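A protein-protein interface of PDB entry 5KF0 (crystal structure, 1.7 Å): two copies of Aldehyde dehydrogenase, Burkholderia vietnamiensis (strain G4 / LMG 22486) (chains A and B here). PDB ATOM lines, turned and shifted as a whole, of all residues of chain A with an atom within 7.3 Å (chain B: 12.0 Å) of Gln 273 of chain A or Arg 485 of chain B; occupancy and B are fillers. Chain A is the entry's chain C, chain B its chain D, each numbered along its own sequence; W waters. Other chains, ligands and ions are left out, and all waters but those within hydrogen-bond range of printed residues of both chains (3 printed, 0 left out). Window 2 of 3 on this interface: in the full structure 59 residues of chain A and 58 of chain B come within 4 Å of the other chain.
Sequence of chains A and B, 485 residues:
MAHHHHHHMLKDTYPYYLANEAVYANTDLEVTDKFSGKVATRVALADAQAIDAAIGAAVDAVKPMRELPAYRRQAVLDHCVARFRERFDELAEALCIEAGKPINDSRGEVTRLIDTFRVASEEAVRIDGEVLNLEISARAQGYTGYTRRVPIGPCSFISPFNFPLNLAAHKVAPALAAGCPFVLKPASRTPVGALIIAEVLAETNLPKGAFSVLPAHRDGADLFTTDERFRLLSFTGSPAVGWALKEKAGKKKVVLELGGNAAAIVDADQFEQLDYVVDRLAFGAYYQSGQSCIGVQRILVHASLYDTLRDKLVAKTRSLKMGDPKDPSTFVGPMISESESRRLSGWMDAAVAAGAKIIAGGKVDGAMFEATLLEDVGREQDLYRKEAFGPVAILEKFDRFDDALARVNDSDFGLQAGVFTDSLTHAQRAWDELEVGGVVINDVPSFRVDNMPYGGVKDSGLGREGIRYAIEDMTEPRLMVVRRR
No residue of chain B comes within 4 Å of Gln 270 of chain A. No residue of chain B comes within 4 Å of Phe 271 of chain A. Of the printed residues of chain B, Gln 273 of chain A touches Arg 485 (3.2 Å). No residue of chain B comes within 4 Å of Leu 274 of chain A. No residue of chain B comes within 4 Å of Val 277 of chain A. Printed residues of chain B within 4 Å of Arg 280 of chain A: Arg 483 (3.7 Å). Of the printed residues of chain A, Arg 483 of chain B touches Tyr 276 (3.0 Å), Arg 280 (3.7 Å) and Asn 442 (3.1 Å). Printed residues of chain A within 4 Å of Arg 485 of chain B: Gln 273, Tyr 276 and Asn 442. The nearest printed residue of chain B that does not touch Gln 273 of chain A is Arg 484 of chain B (9.3 Å). The nearest printed residue of chain A that does not touch Arg 485 of chain B is Val 277 of chain A (6.4 Å).
Of the 16 printed residues of chain A, 4 touch a printed residue of chain B. Hydrophobic or aromatic side chains of chain A that line the printed part of chain B: Tyr 276. Along chain A the printed residues that touch a printed residue of chain B span positions 273 to 442. Printed residues of chain B that touch a printed residue of chain A: Arg 483 and Arg 485. Among the printed residues, 6 pairs touch across the chains. Among the printed residues, no Asp or Glu carboxylate lies within 4 Å of a Lys or Arg side-chain nitrogen of the other chain.
The side-chain amide oxygen of Gln 273 of chain A sits at hydrogen-bond distance from the guanidinium group of Arg 485 of chain B. The guanidinium group (NH1) of Arg 483 of chain B sits at hydrogen-bond distance from the side-chain hydroxyl (OH) of Tyr 276 of chain A. The side-chain amide nitrogen (ND2) of Asn 442 of chain A is in hydrogen-bond range of the backbone carbonyl oxygen (O) of Arg 483 of chain B (3.1 Å).
Water W2 bridges ND2 of Asn 442 of chain A (2.5 Å) and NH1 of Arg 485 of chain B (3.1 Å). Water W1 lies within hydrogen-bond range of the side-chain amide oxygen of Gln 273 of chain A (2.5 Å) and the guanidinium group of Arg 485 of chain B (3.1 Å). Water W3 lies within hydrogen-bond range of the guanidinium group of Arg 483 of chain B and the guanidinium group of Arg 280 of chain A.
OH of Tyr 276 of chain A lies within hydrogen-bond range of O of Asn 442 of chain A (2.7 Å). The side-chain hydroxyl of Tyr 143 of chain B sits close to the guanidinium group of Arg 483 of chain B, 3.2 Å away.
Among the printed residues, merely in contact across the chains: Tyr 276 of chain A with Arg 485 of chain B, Arg 280 of chain A with Arg 483 of chain B and Asn 442 of chain A with Arg 485 of chain B.
No position is printed for both chains. Of the 6 pairs that touch across the chains among the printed residues, none has its exchanged pair printed and touching as well.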
ATOM      1  N   ASP A 269      17.784 -17.472  23.777  1.00  0.00           N
ATOM      2  CA  ASP A 269      16.909 -18.511  23.234  1.00  0.00           C
ATOM      3  C   ASP A 269      17.637 -19.814  22.894  1.00  0.00           C
ATOM      4  O   ASP A 269      17.061 -20.668  22.213  1.00  0.00           O
ATOM      5  CB  ASP A 269      16.180 -17.993  21.979  1.00  0.00           C
ATOM      6  CG  ASP A 269      17.136 -17.535  20.874  1.00  0.00           C
ATOM      7  OD1 ASP A 269      18.371 -17.670  21.023  1.00  0.00           O
ATOM      8  OD2 ASP A 269      16.644 -17.045  19.829  1.00  0.00           O
ATOM      9  N   GLN A 270      18.874 -19.994  23.362  1.00  0.00           N
ATOM     10  CA  GLN A 270      19.733 -21.082  22.904  1.00  0.00           C
ATOM     11  C   GLN A 270      19.758 -22.296  23.831  1.00  0.00           C
ATOM     12  O   GLN A 270      20.577 -23.196  23.610  1.00  0.00           O
ATOM     13  CB  GLN A 270      21.161 -20.562  22.715  1.00  0.00           C
ATOM     14  CG  GLN A 270      21.296 -19.579  21.572  1.00  0.00           C
ATOM     15  CD  GLN A 270      20.953 -20.232  20.264  1.00  0.00           C
ATOM     16  OE1 GLN A 270      21.634 -21.167  19.837  1.00  0.00           O
ATOM     17  NE2 GLN A 270      19.868 -19.776  19.631  1.00  0.00           N
ATOM     18  N   PHE A 271      18.884 -22.364  24.839  1.00  0.00           N
ATOM     19  CA  PHE A 271      19.005 -23.431  25.833  1.00  0.00           C
ATOM     20  C   PHE A 271      18.989 -24.816  25.187  1.00  0.00           C
ATOM     21  O   PHE A 271      19.830 -25.669  25.498  1.00  0.00           O
ATOM     22  CB  PHE A 271      17.897 -23.335  26.879  1.00  0.00           C
ATOM     23  CG  PHE A 271      18.015 -24.390  27.942  1.00  0.00           C
ATOM     24  CD1 PHE A 271      18.908 -24.228  28.987  1.00  0.00           C
ATOM     25  CD2 PHE A 271      17.280 -25.560  27.864  1.00  0.00           C
ATOM     26  CE1 PHE A 271      19.043 -25.201  29.961  1.00  0.00           C
ATOM     27  CE2 PHE A 271      17.411 -26.538  28.833  1.00  0.00           C
ATOM     28  CZ  PHE A 271      18.294 -26.355  29.883  1.00  0.00           C
ATOM     29  N   GLU A 272      18.043 -25.058  24.281  1.00  0.00           N
ATOM     30  CA  GLU A 272      17.909 -26.393  23.715  1.00  0.00           C
ATOM     31  C   GLU A 272      19.068 -26.765  22.800  1.00  0.00           C
ATOM     32  O   GLU A 272      19.228 -27.949  22.486  1.00  0.00           O
ATOM     33  CB  GLU A 272      16.590 -26.523  22.950  1.00  0.00           C
ATOM     34  CG  GLU A 272      15.354 -26.468  23.828  1.00  0.00           C
ATOM     35  CD  GLU A 272      15.347 -27.548  24.890  1.00  0.00           C
ATOM     36  OE1 GLU A 272      15.834 -28.667  24.611  1.00  0.00           O
ATOM     37  OE2 GLU A 272      14.861 -27.276  26.009  1.00  0.00           O
ATOM     38  N   GLN A 273      19.876 -25.802  22.361  1.00  0.00           N
ATOM     39  CA  GLN A 273      20.996 -25.970  21.453  1.00  0.00           C
ATOM     40  C   GLN A 273      22.345 -25.883  22.150  1.00  0.00           C
ATOM     41  O   GLN A 273      23.356 -25.736  21.461  1.00  0.00           O
ATOM     42  CB  GLN A 273      20.949 -24.893  20.362  1.00  0.00           C
ATOM     43  CG  GLN A 273      19.570 -24.605  19.825  1.00  0.00           C
ATOM     44  CD  GLN A 273      18.976 -25.809  19.153  1.00  0.00           C
ATOM     45  OE1 GLN A 273      19.675 -26.558  18.475  1.00  0.00           O
ATOM     46  NE2 GLN A 273      17.680 -26.014  19.345  1.00  0.00           N
ATOM     47  N   LEU A 274      22.392 -25.894  23.485  1.00  0.00           N
ATOM     48  CA  LEU A 274      23.642 -25.551  24.166  1.00  0.00           C
ATOM     49  C   LEU A 274      24.778 -26.507  23.811  1.00  0.00           C
ATOM     50  O   LEU A 274      25.931 -26.084  23.702  1.00  0.00           O
ATOM     51  CB  LEU A 274      23.435 -25.503  25.679  1.00  0.00           C
ATOM     52  CG  LEU A 274      22.853 -24.173  26.177  1.00  0.00           C
ATOM     53  CD1 LEU A 274      22.767 -24.165  27.705  1.00  0.00           C
ATOM     54  CD2 LEU A 274      23.662 -22.980  25.668  1.00  0.00           C
ATOM     55  N   ASP A 275      24.486 -27.804  23.640  1.00  0.00           N
ATOM     56  CA  ASP A 275      25.567 -28.730  23.305  1.00  0.00           C
ATOM     57  C   ASP A 275      26.154 -28.428  21.930  1.00  0.00           C
ATOM     58  O   ASP A 275      27.375 -28.514  21.739  1.00  0.00           O
ATOM     59  CB  ASP A 275      25.073 -30.174  23.374  1.00  0.00           C
ATOM     60  CG  ASP A 275      24.819 -30.633  24.802  1.00  0.00           C
ATOM     61  OD1 ASP A 275      25.485 -30.123  25.729  1.00  0.00           O
ATOM     62  OD2 ASP A 275      23.955 -31.505  24.998  1.00  0.00           O
ATOM     63  N   TYR A 276      25.306 -28.075  20.960  1.00  0.00           N
ATOM     64  CA  TYR A 276      25.802 -27.623  19.663  1.00  0.00           C
ATOM     65  C   TYR A 276      26.625 -26.348  19.811  1.00  0.00           C
ATOM     66  O   TYR A 276      27.730 -26.236  19.265  1.00  0.00           O
ATOM     67  CB  TYR A 276      24.634 -27.391  18.694  1.00  0.00           C
ATOM     68  CG  TYR A 276      25.050 -26.548  17.512  1.00  0.00           C
ATOM     69  CD1 TYR A 276      25.880 -27.070  16.533  1.00  0.00           C
ATOM     70  CD2 TYR A 276      24.647 -25.215  17.390  1.00  0.00           C
ATOM     71  CE1 TYR A 276      26.297 -26.305  15.461  1.00  0.00           C
ATOM     72  CE2 TYR A 276      25.059 -24.437  16.317  1.00  0.00           C
ATOM     73  CZ  TYR A 276      25.889 -24.986  15.359  1.00  0.00           C
ATOM     74  OH  TYR A 276      26.316 -24.248  14.282  1.00  0.00           O
ATOM     75  N   VAL A 277      26.089 -25.369  20.541  1.00  0.00           N
ATOM     76  CA  VAL A 277      26.784 -24.095  20.721  1.00  0.00           C
ATOM     77  C   VAL A 277      28.148 -24.318  21.365  1.00  0.00           C
ATOM     78  O   VAL A 277      29.165 -23.779  20.911  1.00  0.00           O
ATOM     79  CB  VAL A 277      25.923 -23.131  21.556  1.00  0.00           C
ATOM     80  CG1 VAL A 277      26.727 -21.858  21.872  1.00  0.00           C
ATOM     81  CG2 VAL A 277      24.613 -22.798  20.815  1.00  0.00           C
ATOM     82  N   VAL A 278      28.189 -25.134  22.425  1.00  0.00           N
ATOM     83  CA  VAL A 278      29.438 -25.361  23.149  1.00  0.00           C
ATOM     84  C   VAL A 278      30.461 -26.051  22.255  1.00  0.00           C
ATOM     85  O   VAL A 278      31.654 -25.716  22.280  1.00  0.00           O
ATOM     86  CB  VAL A 278      29.159 -26.164  24.434  1.00  0.00           C
ATOM     87  CG1 VAL A 278      30.447 -26.808  24.968  1.00  0.00           C
ATOM     88  CG2 VAL A 278      28.525 -25.259  25.490  1.00  0.00           C
ATOM     89  N   ASP A 279      30.013 -27.019  21.451  1.00  0.00           N
ATOM     90  CA  ASP A 279      30.921 -27.685  20.521  1.00  0.00           C
ATOM     91  C   ASP A 279      31.536 -26.694  19.539  1.00  0.00           C
ATOM     92  O   ASP A 279      32.746 -26.727  19.285  1.00  0.00           O
ATOM     93  CB  ASP A 279      30.186 -28.785  19.762  1.00  0.00           C
ATOM     94  CG  ASP A 279      31.115 -29.579  18.870  1.00  0.00           C
ATOM     95  OD1 ASP A 279      31.968 -30.312  19.413  1.00  0.00           O
ATOM     96  OD2 ASP A 279      31.005 -29.461  17.633  1.00  0.00           O
ATOM     97  N   ARG A 280      30.720 -25.785  18.994  1.00  0.00           N
ATOM     98  CA  ARG A 280      31.250 -24.813  18.042  1.00  0.00           C
ATOM     99  C   ARG A 280      32.132 -23.780  18.734  1.00  0.00           C
ATOM    100  O   ARG A 280      33.125 -23.324  18.156  1.00  0.00           O
ATOM    101  CB  ARG A 280      30.102 -24.123  17.290  1.00  0.00           C
ATOM    102  CG  ARG A 280      29.284 -25.083  16.432  1.00  0.00           C
ATOM    103  CD  ARG A 280      30.202 -25.885  15.501  1.00  0.00           C
ATOM    104  NE  ARG A 280      30.720 -25.036  14.428  1.00  0.00           N
ATOM    105  CZ  ARG A 280      31.730 -25.351  13.617  1.00  0.00           C
ATOM    106  NH1 ARG A 280      32.383 -26.506  13.756  1.00  0.00           N
ATOM    107  NH2 ARG A 280      32.083 -24.503  12.655  1.00  0.00           N
ATOM    108  N   LYS A 312      29.057 -26.693  30.839  1.00  0.00           N
ATOM    109  CA  LYS A 312      29.272 -27.498  29.639  1.00  0.00           C
ATOM    110  C   LYS A 312      30.562 -27.109  28.928  1.00  0.00           C
ATOM    111  O   LYS A 312      31.304 -27.980  28.456  1.00  0.00           O
ATOM    112  CB  LYS A 312      28.086 -27.346  28.684  1.00  0.00           C
ATOM    113  CG  LYS A 312      26.804 -28.029  29.143  1.00  0.00           C
ATOM    114  CD  LYS A 312      25.652 -27.702  28.188  1.00  0.00           C
ATOM    115  CE  LYS A 312      24.391 -28.449  28.590  1.00  0.00           C
ATOM    116  NZ  LYS A 312      24.569 -29.920  28.430  1.00  0.00           N
ATOM    117  N   PHE A 420      24.747 -16.706  18.106  1.00  0.00           N
ATOM    118  CA  PHE A 420      23.845 -17.855  18.199  1.00  0.00           C
ATOM    119  C   PHE A 420      22.494 -17.327  18.675  1.00  0.00           C
ATOM    120  O   PHE A 420      22.324 -16.992  19.847  1.00  0.00           O
ATOM    121  CB  PHE A 420      24.398 -18.917  19.152  1.00  0.00           C
ATOM    122  CG  PHE A 420      25.678 -19.569  18.682  1.00  0.00           C
ATOM    123  CD1 PHE A 420      25.644 -20.705  17.873  1.00  0.00           C
ATOM    124  CD2 PHE A 420      26.908 -19.064  19.066  1.00  0.00           C
ATOM    125  CE1 PHE A 420      26.812 -21.312  17.442  1.00  0.00           C
ATOM    126  CE2 PHE A 420      28.088 -19.662  18.637  1.00  0.00           C
ATOM    127  CZ  PHE A 420      28.038 -20.792  17.819  1.00  0.00           C
ATOM    128  N   ASP A 422      17.980 -17.483  17.444  1.00  0.00           N
ATOM    129  CA  ASP A 422      16.898 -17.776  16.505  1.00  0.00           C
ATOM    130  C   ASP A 422      16.005 -16.560  16.283  1.00  0.00           C
ATOM    131  O   ASP A 422      14.963 -16.669  15.625  1.00  0.00           O
ATOM    132  CB  ASP A 422      16.048 -18.960  16.980  1.00  0.00           C
ATOM    133  CG  ASP A 422      15.066 -19.447  15.904  1.00  0.00           C
ATOM    134  OD1 ASP A 422      15.522 -19.689  14.776  1.00  0.00           O
ATOM    135  OD2 ASP A 422      13.853 -19.563  16.185  1.00  0.00           O
ATOM    136  N   ASN A 442      24.314 -18.270  13.964  1.00  0.00           N
ATOM    137  CA  ASN A 442      24.168 -19.682  14.329  1.00  0.00           C
ATOM    138  C   ASN A 442      25.435 -20.490  14.065  1.00  0.00           C
ATOM    139  O   ASN A 442      25.369 -21.719  13.910  1.00  0.00           O
ATOM    140  CB  ASN A 442      22.965 -20.342  13.630  1.00  0.00           C
ATOM    141  CG  ASN A 442      22.420 -21.530  14.405  1.00  0.00           C
ATOM    142  OD1 ASN A 442      22.527 -21.572  15.624  1.00  0.00           O
ATOM    143  ND2 ASN A 442      21.847 -22.512  13.698  1.00  0.00           N
ATOM    144  N   GLU B 135      26.862 -23.090  -0.449  1.00  0.00           N
ATOM    145  CA  GLU B 135      26.903 -24.554  -0.382  1.00  0.00           C
ATOM    146  C   GLU B 135      27.737 -25.099  -1.542  1.00  0.00           C
ATOM    147  O   GLU B 135      27.233 -25.693  -2.497  1.00  0.00           O
ATOM    148  CB  GLU B 135      25.493 -25.133  -0.393  1.00  0.00           C
ATOM    149  CG  GLU B 135      24.658 -24.736   0.830  1.00  0.00           C
ATOM    150  CD  GLU B 135      23.331 -25.471   0.891  1.00  0.00           C
ATOM    151  OE1 GLU B 135      22.514 -25.327  -0.039  1.00  0.00           O
ATOM    152  OE2 GLU B 135      23.102 -26.209   1.860  1.00  0.00           O
ATOM    153  N   ALA B 138      30.364 -30.100   1.177  1.00  0.00           N
ATOM    154  CA  ALA B 138      29.617 -30.671   2.294  1.00  0.00           C
ATOM    155  C   ALA B 138      29.863 -29.905   3.593  1.00  0.00           C
ATOM    156  O   ALA B 138      28.943 -29.746   4.407  1.00  0.00           O
ATOM    157  CB  ALA B 138      29.979 -32.145   2.462  1.00  0.00           C
ATOM    158  N   ARG B 139      31.093 -29.429   3.807  1.00  0.00           N
ATOM    159  CA  ARG B 139      31.408 -28.659   5.009  1.00  0.00           C
ATOM    160  C   ARG B 139      30.531 -27.417   5.125  1.00  0.00           C
ATOM    161  O   ARG B 139      30.184 -27.002   6.239  1.00  0.00           O
ATOM    162  CB  ARG B 139      32.888 -28.266   4.994  1.00  0.00           C
ATOM    163  CG  ARG B 139      33.411 -27.598   6.259  1.00  0.00           C
ATOM    164  CD  ARG B 139      34.892 -27.229   6.104  1.00  0.00           C
ATOM    165  NE  ARG B 139      35.088 -26.215   5.073  1.00  0.00           N
ATOM    166  CZ  ARG B 139      35.071 -24.910   5.318  1.00  0.00           C
ATOM    167  NH1 ARG B 139      34.888 -24.467   6.556  1.00  0.00           N
ATOM    168  NH2 ARG B 139      35.237 -24.049   4.327  1.00  0.00           N
ATOM    169  N   ALA B 140      30.164 -26.811   3.995  1.00  0.00           N
ATOM    170  CA  ALA B 140      29.360 -25.596   3.981  1.00  0.00           C
ATOM    171  C   ALA B 140      27.878 -25.876   3.729  1.00  0.00           C
ATOM    172  O   ALA B 140      27.128 -24.950   3.385  1.00  0.00           O
ATOM    173  CB  ALA B 140      29.907 -24.622   2.936  1.00  0.00           C
ATOM    174  N   GLN B 141      27.437 -27.122   3.904  1.00  0.00           N
ATOM    175  CA  GLN B 141      26.019 -27.421   3.753  1.00  0.00           C
ATOM    176  C   GLN B 141      25.214 -26.640   4.782  1.00  0.00           C
ATOM    177  O   GLN B 141      25.555 -26.626   5.969  1.00  0.00           O
ATOM    178  CB  GLN B 141      25.741 -28.919   3.928  1.00  0.00           C
ATOM    179  CG  GLN B 141      24.274 -29.236   3.637  1.00  0.00           C
ATOM    180  CD  GLN B 141      23.920 -30.711   3.725  1.00  0.00           C
ATOM    181  OE1 GLN B 141      24.699 -31.525   4.210  1.00  0.00           O
ATOM    182  NE2 GLN B 141      22.727 -31.058   3.253  1.00  0.00           N
ATOM    183  N   GLY B 142      24.144 -25.993   4.324  1.00  0.00           N
ATOM    184  CA  GLY B 142      23.282 -25.262   5.224  1.00  0.00           C
ATOM    185  C   GLY B 142      23.665 -23.821   5.472  1.00  0.00           C
ATOM    186  O   GLY B 142      22.974 -23.143   6.238  1.00  0.00           O
ATOM    187  N   TYR B 143      24.726 -23.317   4.852  1.00  0.00           N
ATOM    188  CA  TYR B 143      25.103 -21.919   5.018  1.00  0.00           C
ATOM    189  C   TYR B 143      24.697 -21.115   3.791  1.00  0.00           C
ATOM    190  O   TYR B 143      24.838 -21.588   2.658  1.00  0.00           O
ATOM    191  CB  TYR B 143      26.604 -21.766   5.215  1.00  0.00           C
ATOM    192  CG  TYR B 143      27.221 -22.380   6.453  1.00  0.00           C
ATOM    193  CD1 TYR B 143      27.629 -21.578   7.513  1.00  0.00           C
ATOM    194  CD2 TYR B 143      27.468 -23.746   6.527  1.00  0.00           C
ATOM    195  CE1 TYR B 143      28.239 -22.131   8.636  1.00  0.00           C
ATOM    196  CE2 TYR B 143      28.088 -24.309   7.648  1.00  0.00           C
ATOM    197  CZ  TYR B 143      28.474 -23.486   8.694  1.00  0.00           C
ATOM    198  OH  TYR B 143      29.101 -24.034   9.793  1.00  0.00           O
ATOM    199  N   THR B 144      24.232 -19.885   4.024  1.00  0.00           N
ATOM    200  CA  THR B 144      23.888 -18.935   2.971  1.00  0.00           C
ATOM    201  C   THR B 144      24.469 -17.575   3.328  1.00  0.00           C
ATOM    202  O   THR B 144      24.537 -17.215   4.504  1.00  0.00           O
ATOM    203  CB  THR B 144      22.356 -18.812   2.802  1.00  0.00           C
ATOM    204  OG1 THR B 144      21.789 -20.107   2.590  1.00  0.00           O
ATOM    205  CG2 THR B 144      22.006 -17.914   1.599  1.00  0.00           C
ATOM    206  N   TYR B 146      24.483 -13.277   2.785  1.00  0.00           N
ATOM    207  CA  TYR B 146      23.677 -12.099   2.477  1.00  0.00           C
ATOM    208  C   TYR B 146      24.589 -10.890   2.584  1.00  0.00           C
ATOM    209  O   TYR B 146      25.296 -10.750   3.588  1.00  0.00           O
ATOM    210  CB  TYR B 146      22.503 -11.955   3.460  1.00  0.00           C
ATOM    211  CG  TYR B 146      21.575 -13.148   3.464  1.00  0.00           C
ATOM    212  CD1 TYR B 146      20.460 -13.188   2.634  1.00  0.00           C
ATOM    213  CD2 TYR B 146      21.834 -14.250   4.273  1.00  0.00           C
ATOM    214  CE1 TYR B 146      19.616 -14.290   2.625  1.00  0.00           C
ATOM    215  CE2 TYR B 146      20.991 -15.353   4.276  1.00  0.00           C
ATOM    216  CZ  TYR B 146      19.891 -15.366   3.447  1.00  0.00           C
ATOM    217  OH  TYR B 146      19.069 -16.461   3.447  1.00  0.00           O
ATOM    218  N   VAL B 481      26.461 -14.360   7.223  1.00  0.00           N
ATOM    219  CA  VAL B 481      26.380 -15.793   6.947  1.00  0.00           C
ATOM    220  C   VAL B 481      25.351 -16.379   7.894  1.00  0.00           C
ATOM    221  O   VAL B 481      25.468 -16.217   9.108  1.00  0.00           O
ATOM    222  CB  VAL B 481      27.742 -16.482   7.148  1.00  0.00           C
ATOM    223  CG1 VAL B 481      27.607 -17.995   6.961  1.00  0.00           C
ATOM    224  CG2 VAL B 481      28.779 -15.912   6.200  1.00  0.00           C
ATOM    225  N   VAL B 482      24.350 -17.077   7.362  1.00  0.00           N
ATOM    226  CA  VAL B 482      23.339 -17.713   8.207  1.00  0.00           C
ATOM    227  C   VAL B 482      23.477 -19.220   8.058  1.00  0.00           C
ATOM    228  O   VAL B 482      23.424 -19.744   6.936  1.00  0.00           O
ATOM    229  CB  VAL B 482      21.921 -17.250   7.836  1.00  0.00           C
ATOM    230  CG1 VAL B 482      20.894 -17.889   8.765  1.00  0.00           C
ATOM    231  CG2 VAL B 482      21.820 -15.720   7.883  1.00  0.00           C
ATOM    232  N   ARG B 483      23.655 -19.921   9.181  1.00  0.00           N
ATOM    233  CA  ARG B 483      23.732 -21.379   9.185  1.00  0.00           C
ATOM    234  C   ARG B 483      22.398 -21.971   9.620  1.00  0.00           C
ATOM    235  O   ARG B 483      21.878 -21.636  10.692  1.00  0.00           O
ATOM    236  CB  ARG B 483      24.831 -21.903  10.113  1.00  0.00           C
ATOM    237  CG  ARG B 483      25.035 -23.424   9.940  1.00  0.00           C
ATOM    238  CD  ARG B 483      25.900 -24.084  11.004  1.00  0.00           C
ATOM    239  NE  ARG B 483      26.329 -25.391  10.506  1.00  0.00           N
ATOM    240  CZ  ARG B 483      27.244 -26.159  11.083  1.00  0.00           C
ATOM    241  NH1 ARG B 483      27.809 -25.784  12.220  1.00  0.00           N
ATOM    242  NH2 ARG B 483      27.591 -27.308  10.517  1.00  0.00           N
ATOM    243  N   ARG B 484      21.860 -22.858   8.789  1.00  0.00           N
ATOM    244  CA  ARG B 484      20.712 -23.682   9.135  1.00  0.00           C
ATOM    245  C   ARG B 484      21.200 -25.102   9.374  1.00  0.00           C
ATOM    246  O   ARG B 484      22.026 -25.622   8.615  1.00  0.00           O
ATOM    247  CB  ARG B 484      19.677 -23.659   8.012  1.00  0.00           C
ATOM    248  CG  ARG B 484      19.198 -22.259   7.691  1.00  0.00           C
ATOM    249  CD  ARG B 484      18.255 -22.268   6.515  1.00  0.00           C
ATOM    250  NE  ARG B 484      17.041 -23.022   6.804  1.00  0.00           N
ATOM    251  CZ  ARG B 484      16.159 -23.371   5.874  1.00  0.00           C
ATOM    252  NH1 ARG B 484      16.376 -23.036   4.607  1.00  0.00           N
ATOM    253  NH2 ARG B 484      15.071 -24.054   6.206  1.00  0.00           N
ATOM    254  N   ARG B 485      20.692 -25.732  10.421  1.00  0.00           N
ATOM    255  CA  ARG B 485      21.101 -27.103  10.688  1.00  0.00           C
ATOM    256  C   ARG B 485      19.936 -27.928  11.211  1.00  0.00           C
ATOM    257  O   ARG B 485      18.898 -27.378  11.583  1.00  0.00           O
ATOM    258  CB  ARG B 485      22.266 -27.122  11.674  1.00  0.00           C
ATOM    259  CG  ARG B 485      22.074 -26.198  12.852  1.00  0.00           C
ATOM    260  CD  ARG B 485      23.183 -26.373  13.852  1.00  0.00           C
ATOM    261  NE  ARG B 485      23.184 -27.708  14.440  1.00  0.00           N
ATOM    262  CZ  ARG B 485      22.507 -28.040  15.539  1.00  0.00           C
ATOM    263  NH1 ARG B 485      21.774 -27.136  16.174  1.00  0.00           N
ATOM    264  NH2 ARG B 485      22.572 -29.278  16.011  1.00  0.00           N
ATOM    265  OXT ARG B 485      20.012 -29.158  11.250  1.00  0.00           O
HETATM  266  O   HOH W   1      20.849 -28.783  18.596  1.00  0.00           O
HETATM  267  O   HOH W   2      21.098 -24.216  15.304  1.00  0.00           O
HETATM  268  O   HOH W   3      29.576 -28.040  12.587  1.00  0.00           O
